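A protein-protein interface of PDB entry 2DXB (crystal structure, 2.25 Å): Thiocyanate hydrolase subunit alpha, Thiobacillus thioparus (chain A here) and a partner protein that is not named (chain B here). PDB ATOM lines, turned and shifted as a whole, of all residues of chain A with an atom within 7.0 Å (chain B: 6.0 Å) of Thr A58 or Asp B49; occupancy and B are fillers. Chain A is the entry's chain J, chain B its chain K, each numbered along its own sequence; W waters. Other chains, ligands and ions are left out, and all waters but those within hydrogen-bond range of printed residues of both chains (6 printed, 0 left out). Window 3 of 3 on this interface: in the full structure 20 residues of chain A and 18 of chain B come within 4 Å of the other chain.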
ATOM      1  N   ASP A  47      20.519  19.900 -24.757  1.00  0.00           N
ATOM      2  CA  ASP A  47      19.478  19.126 -24.105  1.00  0.00           C
ATOM      3  C   ASP A  47      18.608  20.029 -23.242  1.00  0.00           C
ATOM      4  O   ASP A  47      18.620  19.944 -22.016  1.00  0.00           O
ATOM      5  CB  ASP A  47      20.095  18.011 -23.262  1.00  0.00           C
ATOM      6  CG  ASP A  47      19.051  17.069 -22.704  1.00  0.00           C
ATOM      7  OD1 ASP A  47      17.966  16.967 -23.319  1.00  0.00           O
ATOM      8  OD2 ASP A  47      19.315  16.426 -21.664  1.00  0.00           O
ATOM      9  N   ASP A  50      12.406  19.646 -21.698  1.00  0.00           N
ATOM     10  CA  ASP A  50      11.342  19.348 -22.644  1.00  0.00           C
ATOM     11  C   ASP A  50       9.969  19.216 -21.988  1.00  0.00           C
ATOM     12  O   ASP A  50       9.038  18.662 -22.576  1.00  0.00           O
ATOM     13  CB  ASP A  50      11.691  18.069 -23.408  1.00  0.00           C
ATOM     14  CG  ASP A  50      11.840  16.870 -22.497  1.00  0.00           C
ATOM     15  OD1 ASP A  50      12.402  17.032 -21.392  1.00  0.00           O
ATOM     16  OD2 ASP A  50      11.409  15.762 -22.886  1.00  0.00           O
ATOM     17  N   THR A  54       7.853  19.555 -26.964  1.00  0.00           N
ATOM     18  CA  THR A  54       9.070  19.756 -27.737  1.00  0.00           C
ATOM     19  C   THR A  54       8.968  18.949 -29.020  1.00  0.00           C
ATOM     20  O   THR A  54       8.285  17.922 -29.061  1.00  0.00           O
ATOM     21  CB  THR A  54      10.337  19.291 -26.974  1.00  0.00           C
ATOM     22  OG1 THR A  54      11.485  19.461 -27.816  1.00  0.00           O
ATOM     23  CG2 THR A  54      10.230  17.824 -26.588  1.00  0.00           C
ATOM     24  N   ARG A  55       9.628  19.424 -30.071  1.00  0.00           N
ATOM     25  CA  ARG A  55       9.636  18.703 -31.335  1.00  0.00           C
ATOM     26  C   ARG A  55      11.078  18.381 -31.732  1.00  0.00           C
ATOM     27  O   ARG A  55      11.373  18.071 -32.889  1.00  0.00           O
ATOM     28  CB  ARG A  55       8.918  19.495 -32.431  1.00  0.00           C
ATOM     29  CG  ARG A  55       7.400  19.592 -32.192  1.00  0.00           C
ATOM     30  CD  ARG A  55       6.633  20.040 -33.427  1.00  0.00           C
ATOM     31  NE  ARG A  55       6.506  18.983 -34.428  1.00  0.00           N
ATOM     32  CZ  ARG A  55       5.681  17.944 -34.329  1.00  0.00           C
ATOM     33  NH1 ARG A  55       4.890  17.804 -33.263  1.00  0.00           N
ATOM     34  NH2 ARG A  55       5.642  17.044 -35.299  1.00  0.00           N
ATOM     35  N   THR A  56      11.972  18.462 -30.751  1.00  0.00           N
ATOM     36  CA  THR A  56      13.378  18.132 -30.958  1.00  0.00           C
ATOM     37  C   THR A  56      13.552  16.812 -30.215  1.00  0.00           C
ATOM     38  O   THR A  56      13.776  16.793 -28.998  1.00  0.00           O
ATOM     39  CB  THR A  56      14.312  19.199 -30.356  1.00  0.00           C
ATOM     40  OG1 THR A  56      14.083  20.455 -31.006  1.00  0.00           O
ATOM     41  CG2 THR A  56      15.773  18.791 -30.542  1.00  0.00           C
ATOM     42  N   MET A  57      13.425  15.715 -30.958  1.00  0.00           N
ATOM     43  CA  MET A  57      13.505  14.364 -30.409  1.00  0.00           C
ATOM     44  C   MET A  57      14.640  14.082 -29.437  1.00  0.00           C
ATOM     45  O   MET A  57      15.780  14.508 -29.632  1.00  0.00           O
ATOM     46  CB  MET A  57      13.563  13.332 -31.540  1.00  0.00           C
ATOM     47  CG  MET A  57      12.365  13.340 -32.488  1.00  0.00           C
ATOM     48  SD  MET A  57      12.390  14.711 -33.659  1.00  0.00           S
ATOM     49  CE  MET A  57      13.929  14.391 -34.525  1.00  0.00           C
ATOM     50  N   THR A  58      14.310  13.335 -28.391  1.00  0.00           N
ATOM     51  CA  THR A  58      15.277  12.958 -27.376  1.00  0.00           C
ATOM     52  C   THR A  58      16.487  12.247 -27.981  1.00  0.00           C
ATOM     53  O   THR A  58      17.612  12.435 -27.517  1.00  0.00           O
ATOM     54  CB  THR A  58      14.640  12.015 -26.322  1.00  0.00           C
ATOM     55  OG1 THR A  58      13.574  12.695 -25.645  1.00  0.00           O
ATOM     56  CG2 THR A  58      15.686  11.575 -25.297  1.00  0.00           C
ATOM     57  N   TYR A  59      16.273  11.452 -29.026  1.00  0.00           N
ATOM     58  CA  TYR A  59      17.380  10.711 -29.620  1.00  0.00           C
ATOM     59  C   TYR A  59      18.478  11.568 -30.254  1.00  0.00           C
ATOM     60  O   TYR A  59      19.555  11.061 -30.578  1.00  0.00           O
ATOM     61  CB  TYR A  59      16.850   9.656 -30.616  1.00  0.00           C
ATOM     62  CG  TYR A  59      16.387  10.158 -31.970  1.00  0.00           C
ATOM     63  CD1 TYR A  59      17.305  10.550 -32.942  1.00  0.00           C
ATOM     64  CD2 TYR A  59      15.027  10.203 -32.292  1.00  0.00           C
ATOM     65  CE1 TYR A  59      16.884  10.975 -34.201  1.00  0.00           C
ATOM     66  CE2 TYR A  59      14.595  10.629 -33.548  1.00  0.00           C
ATOM     67  CZ  TYR A  59      15.528  11.013 -34.498  1.00  0.00           C
ATOM     68  OH  TYR A  59      15.112  11.447 -35.738  1.00  0.00           O
ATOM     69  N   THR A  60      18.221  12.866 -30.403  1.00  0.00           N
ATOM     70  CA  THR A  60      19.200  13.776 -30.992  1.00  0.00           C
ATOM     71  C   THR A  60      19.972  14.590 -29.956  1.00  0.00           C
ATOM     72  O   THR A  60      20.990  15.196 -30.280  1.00  0.00           O
ATOM     73  CB  THR A  60      18.538  14.795 -31.940  1.00  0.00           C
ATOM     74  OG1 THR A  60      17.751  15.717 -31.172  1.00  0.00           O
ATOM     75  CG2 THR A  60      17.652  14.088 -32.954  1.00  0.00           C
ATOM     76  N   ARG A  61      19.493  14.606 -28.717  1.00  0.00           N
ATOM     77  CA  ARG A  61      20.140  15.391 -27.666  1.00  0.00           C
ATOM     78  C   ARG A  61      21.613  15.054 -27.433  1.00  0.00           C
ATOM     79  O   ARG A  61      21.980  13.893 -27.244  1.00  0.00           O
ATOM     80  CB  ARG A  61      19.372  15.246 -26.347  1.00  0.00           C
ATOM     81  CG  ARG A  61      17.873  15.537 -26.439  1.00  0.00           C
ATOM     82  CD  ARG A  61      17.589  16.848 -27.155  1.00  0.00           C
ATOM     83  NE  ARG A  61      16.160  17.155 -27.231  1.00  0.00           N
ATOM     84  CZ  ARG A  61      15.495  17.879 -26.332  1.00  0.00           C
ATOM     85  NH1 ARG A  61      16.124  18.382 -25.274  1.00  0.00           N
ATOM     86  NH2 ARG A  61      14.200  18.120 -26.501  1.00  0.00           N
ATOM     87  N   GLY A  62      22.451  16.087 -27.445  1.00  0.00           N
ATOM     88  CA  GLY A  62      23.872  15.895 -27.219  1.00  0.00           C
ATOM     89  C   GLY A  62      24.644  15.380 -28.423  1.00  0.00           C
ATOM     90  O   GLY A  62      25.862  15.258 -28.362  1.00  0.00           O
ATOM     91  N   ARG B  41      12.340  12.112 -15.405  1.00  0.00           N
ATOM     92  CA  ARG B  41      12.443  12.433 -16.824  1.00  0.00           C
ATOM     93  C   ARG B  41      11.544  11.515 -17.644  1.00  0.00           C
ATOM     94  O   ARG B  41      10.949  11.940 -18.632  1.00  0.00           O
ATOM     95  CB  ARG B  41      13.891  12.298 -17.303  1.00  0.00           C
ATOM     96  CG  ARG B  41      14.116  12.810 -18.720  1.00  0.00           C
ATOM     97  CD  ARG B  41      15.468  12.383 -19.274  1.00  0.00           C
ATOM     98  NE  ARG B  41      15.674  12.864 -20.639  1.00  0.00           N
ATOM     99  CZ  ARG B  41      16.448  13.896 -20.964  1.00  0.00           C
ATOM    100  NH1 ARG B  41      17.101  14.559 -20.020  1.00  0.00           N
ATOM    101  NH2 ARG B  41      16.561  14.274 -22.233  1.00  0.00           N
ATOM    102  N   ARG B  45       8.168  12.960 -19.674  1.00  0.00           N
ATOM    103  CA  ARG B  45       8.505  12.895 -21.093  1.00  0.00           C
ATOM    104  C   ARG B  45       7.295  13.331 -21.907  1.00  0.00           C
ATOM    105  O   ARG B  45       6.168  13.321 -21.416  1.00  0.00           O
ATOM    106  CB  ARG B  45       8.822  11.454 -21.498  1.00  0.00           C
ATOM    107  CG  ARG B  45       7.554  10.594 -21.520  1.00  0.00           C
ATOM    108  CD  ARG B  45       7.748   9.200 -22.089  1.00  0.00           C
ATOM    109  NE  ARG B  45       8.145   9.224 -23.491  1.00  0.00           N
ATOM    110  CZ  ARG B  45       7.996   8.199 -24.319  1.00  0.00           C
ATOM    111  NH1 ARG B  45       7.450   7.068 -23.889  1.00  0.00           N
ATOM    112  NH2 ARG B  45       8.403   8.300 -25.573  1.00  0.00           N
ATOM    113  N   VAL B  46       7.543  13.691 -23.159  1.00  0.00           N
ATOM    114  CA  VAL B  46       6.484  14.072 -24.078  1.00  0.00           C
ATOM    115  C   VAL B  46       6.153  12.750 -24.790  1.00  0.00           C
ATOM    116  O   VAL B  46       6.996  12.174 -25.482  1.00  0.00           O
ATOM    117  CB  VAL B  46       6.987  15.127 -25.086  1.00  0.00           C
ATOM    118  CG1 VAL B  46       5.837  15.661 -25.882  1.00  0.00           C
ATOM    119  CG2 VAL B  46       7.668  16.268 -24.347  1.00  0.00           C
ATOM    120  N   PRO B  47       4.926  12.246 -24.612  1.00  0.00           N
ATOM    121  CA  PRO B  47       4.452  10.991 -25.204  1.00  0.00           C
ATOM    122  C   PRO B  47       4.777  10.668 -26.668  1.00  0.00           C
ATOM    123  O   PRO B  47       5.129   9.530 -26.980  1.00  0.00           O
ATOM    124  CB  PRO B  47       2.946  11.046 -24.950  1.00  0.00           C
ATOM    125  CG  PRO B  47       2.873  11.750 -23.638  1.00  0.00           C
ATOM    126  CD  PRO B  47       3.842  12.895 -23.853  1.00  0.00           C
ATOM    127  N   HIS B  48       4.672  11.651 -27.557  1.00  0.00           N
ATOM    128  CA  HIS B  48       4.912  11.404 -28.978  1.00  0.00           C
ATOM    129  C   HIS B  48       6.355  11.129 -29.396  1.00  0.00           C
ATOM    130  O   HIS B  48       6.594  10.659 -30.511  1.00  0.00           O
ATOM    131  CB  HIS B  48       4.361  12.567 -29.818  1.00  0.00           C
ATOM    132  CG  HIS B  48       5.113  13.856 -29.658  1.00  0.00           C
ATOM    133  ND1 HIS B  48       4.785  14.996 -30.360  1.00  0.00           N
ATOM    134  CD2 HIS B  48       6.167  14.186 -28.871  1.00  0.00           C
ATOM    135  CE1 HIS B  48       5.603  15.976 -30.012  1.00  0.00           C
ATOM    136  NE2 HIS B  48       6.450  15.511 -29.111  1.00  0.00           N
ATOM    137  N   ASP B  49       7.306  11.407 -28.512  1.00  0.00           N
ATOM    138  CA  ASP B  49       8.727  11.217 -28.813  1.00  0.00           C
ATOM    139  C   ASP B  49       9.150   9.764 -28.587  1.00  0.00           C
ATOM    140  O   ASP B  49       9.715   9.424 -27.550  1.00  0.00           O
ATOM    141  CB  ASP B  49       9.547  12.166 -27.932  1.00  0.00           C
ATOM    142  CG  ASP B  49      11.019  12.189 -28.293  1.00  0.00           C
ATOM    143  OD1 ASP B  49      11.387  11.715 -29.391  1.00  0.00           O
ATOM    144  OD2 ASP B  49      11.810  12.703 -27.473  1.00  0.00           O
ATOM    145  N   VAL B  50       8.888   8.912 -29.574  1.00  0.00           N
ATOM    146  CA  VAL B  50       9.205   7.489 -29.457  1.00  0.00           C
ATOM    147  C   VAL B  50      10.367   6.976 -30.309  1.00  0.00           C
ATOM    148  O   VAL B  50      10.759   5.818 -30.176  1.00  0.00           O
ATOM    149  CB  VAL B  50       7.969   6.638 -29.798  1.00  0.00           C
ATOM    150  CG1 VAL B  50       6.784   7.059 -28.922  1.00  0.00           C
ATOM    151  CG2 VAL B  50       7.625   6.801 -31.283  1.00  0.00           C
ATOM    152  N   GLY B  51      10.913   7.826 -31.174  1.00  0.00           N
ATOM    153  CA  GLY B  51      12.012   7.413 -32.035  1.00  0.00           C
ATOM    154  C   GLY B  51      13.208   6.800 -31.323  1.00  0.00           C
ATOM    155  O   GLY B  51      13.762   7.396 -30.397  1.00  0.00           O
ATOM    156  N   GLU B  53      13.132   3.884 -29.657  1.00  0.00           N
ATOM    157  CA  GLU B  53      12.717   2.907 -28.653  1.00  0.00           C
ATOM    158  C   GLU B  53      12.693   1.531 -29.307  1.00  0.00           C
ATOM    159  O   GLU B  53      12.288   1.391 -30.462  1.00  0.00           O
ATOM    160  CB  GLU B  53      11.321   3.240 -28.112  1.00  0.00           C
ATOM    161  CG  GLU B  53      11.266   4.486 -27.246  1.00  0.00           C
ATOM    162  CD  GLU B  53       9.844   4.904 -26.906  1.00  0.00           C
ATOM    163  OE1 GLU B  53       8.903   4.118 -27.155  1.00  0.00           O
ATOM    164  OE2 GLU B  53       9.666   6.025 -26.385  1.00  0.00           O
ATOM    165  N   TYR B 103      -2.478   7.664 -25.052  1.00  0.00           N
ATOM    166  CA  TYR B 103      -1.657   7.802 -26.246  1.00  0.00           C
ATOM    167  C   TYR B 103      -1.434   6.484 -26.992  1.00  0.00           C
ATOM    168  O   TYR B 103      -1.477   6.442 -28.222  1.00  0.00           O
ATOM    169  CB  TYR B 103      -0.300   8.419 -25.896  1.00  0.00           C
ATOM    170  CG  TYR B 103       0.526   8.699 -27.123  1.00  0.00           C
ATOM    171  CD1 TYR B 103       0.077   9.598 -28.090  1.00  0.00           C
ATOM    172  CD2 TYR B 103       1.721   8.012 -27.356  1.00  0.00           C
ATOM    173  CE1 TYR B 103       0.786   9.806 -29.264  1.00  0.00           C
ATOM    174  CE2 TYR B 103       2.445   8.214 -28.525  1.00  0.00           C
ATOM    175  CZ  TYR B 103       1.971   9.109 -29.478  1.00  0.00           C
ATOM    176  OH  TYR B 103       2.658   9.293 -30.652  1.00  0.00           O
HETATM  177  O   HOH W   1       3.143  15.425 -32.638  1.00  0.00           O
HETATM  178  O   HOH W   2      13.288  13.186 -22.881  1.00  0.00           O
HETATM  179  O   HOH W   3      14.305  15.248 -24.625  1.00  0.00           O
HETATM  180  O   HOH W   4      10.232  13.488 -24.076  1.00  0.00           O
HETATM  181  O   HOH W   5      11.493  14.415 -20.293  1.00  0.00           O
HETATM  182  O   HOH W   6      13.473  10.044 -29.105  1.00  0.00           O
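The side-chain carboxylate of Asp A47 is in salt-bridge range of the guanidinium group of Arg B41.
O of Thr A54 is in hydrogen-bond range of NE2 of His B48, at 3.0 Å.
The side-chain carboxylate of Asp B49 sits at hydrogen-bond distance from the side-chain hydroxyl of Thr A58, at 2.5 Å.
OD1 of Asp A47 lies within salt-bridge range of NH1 of Arg A61 (3.0 Å).
The backbone NH (N) of Thr A56 sits at hydrogen-bond distance from the side-chain hydroxyl (OG1) of Thr A54.
The guanidinium group of Arg A61 is in hydrogen-bond range of the side-chain hydroxyl of Thr A54.
The side-chain hydroxyl (OG1) of Thr A60 sits at hydrogen-bond distance from the backbone carbonyl oxygen (O) of Met A57.
The guanidinium group (NH2) of Arg B45 is in hydrogen-bond range of the backbone carbonyl oxygen (O) of Asp B49, 2.6 Å away.
Val B46 touches Asp A50 (CG2 to O, 3.3 Å).
Thr A54 touches Val B46 (CG2 to CG2, 3.7 Å).
NH1 of Arg A55 touches CE1 of His B48, at 3.8 Å.
Asp B49 touches Met A57 (OD1 to CB, 3.5 Å).
CD2 of Tyr A59 touches O of Gly B51, at 3.6 Å.
Of the printed residues of chain B, Thr A58 touches Asp B49.
Of the printed residues of chain B, Tyr A59 touches Gly B51.
Gly A62 touches none of the printed residues of chain B.
Of the printed residues of chain A, Val B46 touches Asp A50 and Thr A54.
Of the printed residues of chain A, Asp B49 touches Met A57 (3.5 Å) and Thr A58 (2.5 Å).
The nearest residue of chain B that does not touch Thr A58 is Arg B41 (4.2 Å).
The nearest residue of chain A that does not touch Asp B49 is Thr A56 (4.8 Å).
Printed residues of chain A that touch a printed residue of chain B: Asp A47, Asp A50, Thr A54, Arg A55, Met A57, Thr A58 and Tyr A59.
Among the printed residues, 8 pairs touch across the chains.
Water W6 lies within hydrogen-bond range of OD1 of Asp B49, O of Gly B51, N of Tyr A59 and N of Thr A58.
Water W2 lies within hydrogen-bond range of OG1 of Thr A58 (2.8 Å), OD2 of Asp A50 (3.2 Å) and NE of Arg B41 (3.3 Å).
Water W4 bridges the side-chain carboxylate of Asp A50 (2.8 Å) and the backbone NH of Val B46 (2.8 Å).
Water W1 lies within hydrogen-bond range of ND1 of His B48 (2.8 Å) and NH1 of Arg A55 (3.0 Å).
Water W3 lies within hydrogen-bond range of OG1 of Thr A58 (2.8 Å), OD2 of Asp A50 (3.4 Å), NH2 of Arg B41 (3.4 Å) and NH2 of Arg A61 (3.4 Å).
Water W5 bridges OD2 of Asp A50 (2.9 Å) and O of Arg B41 (3.0 Å).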
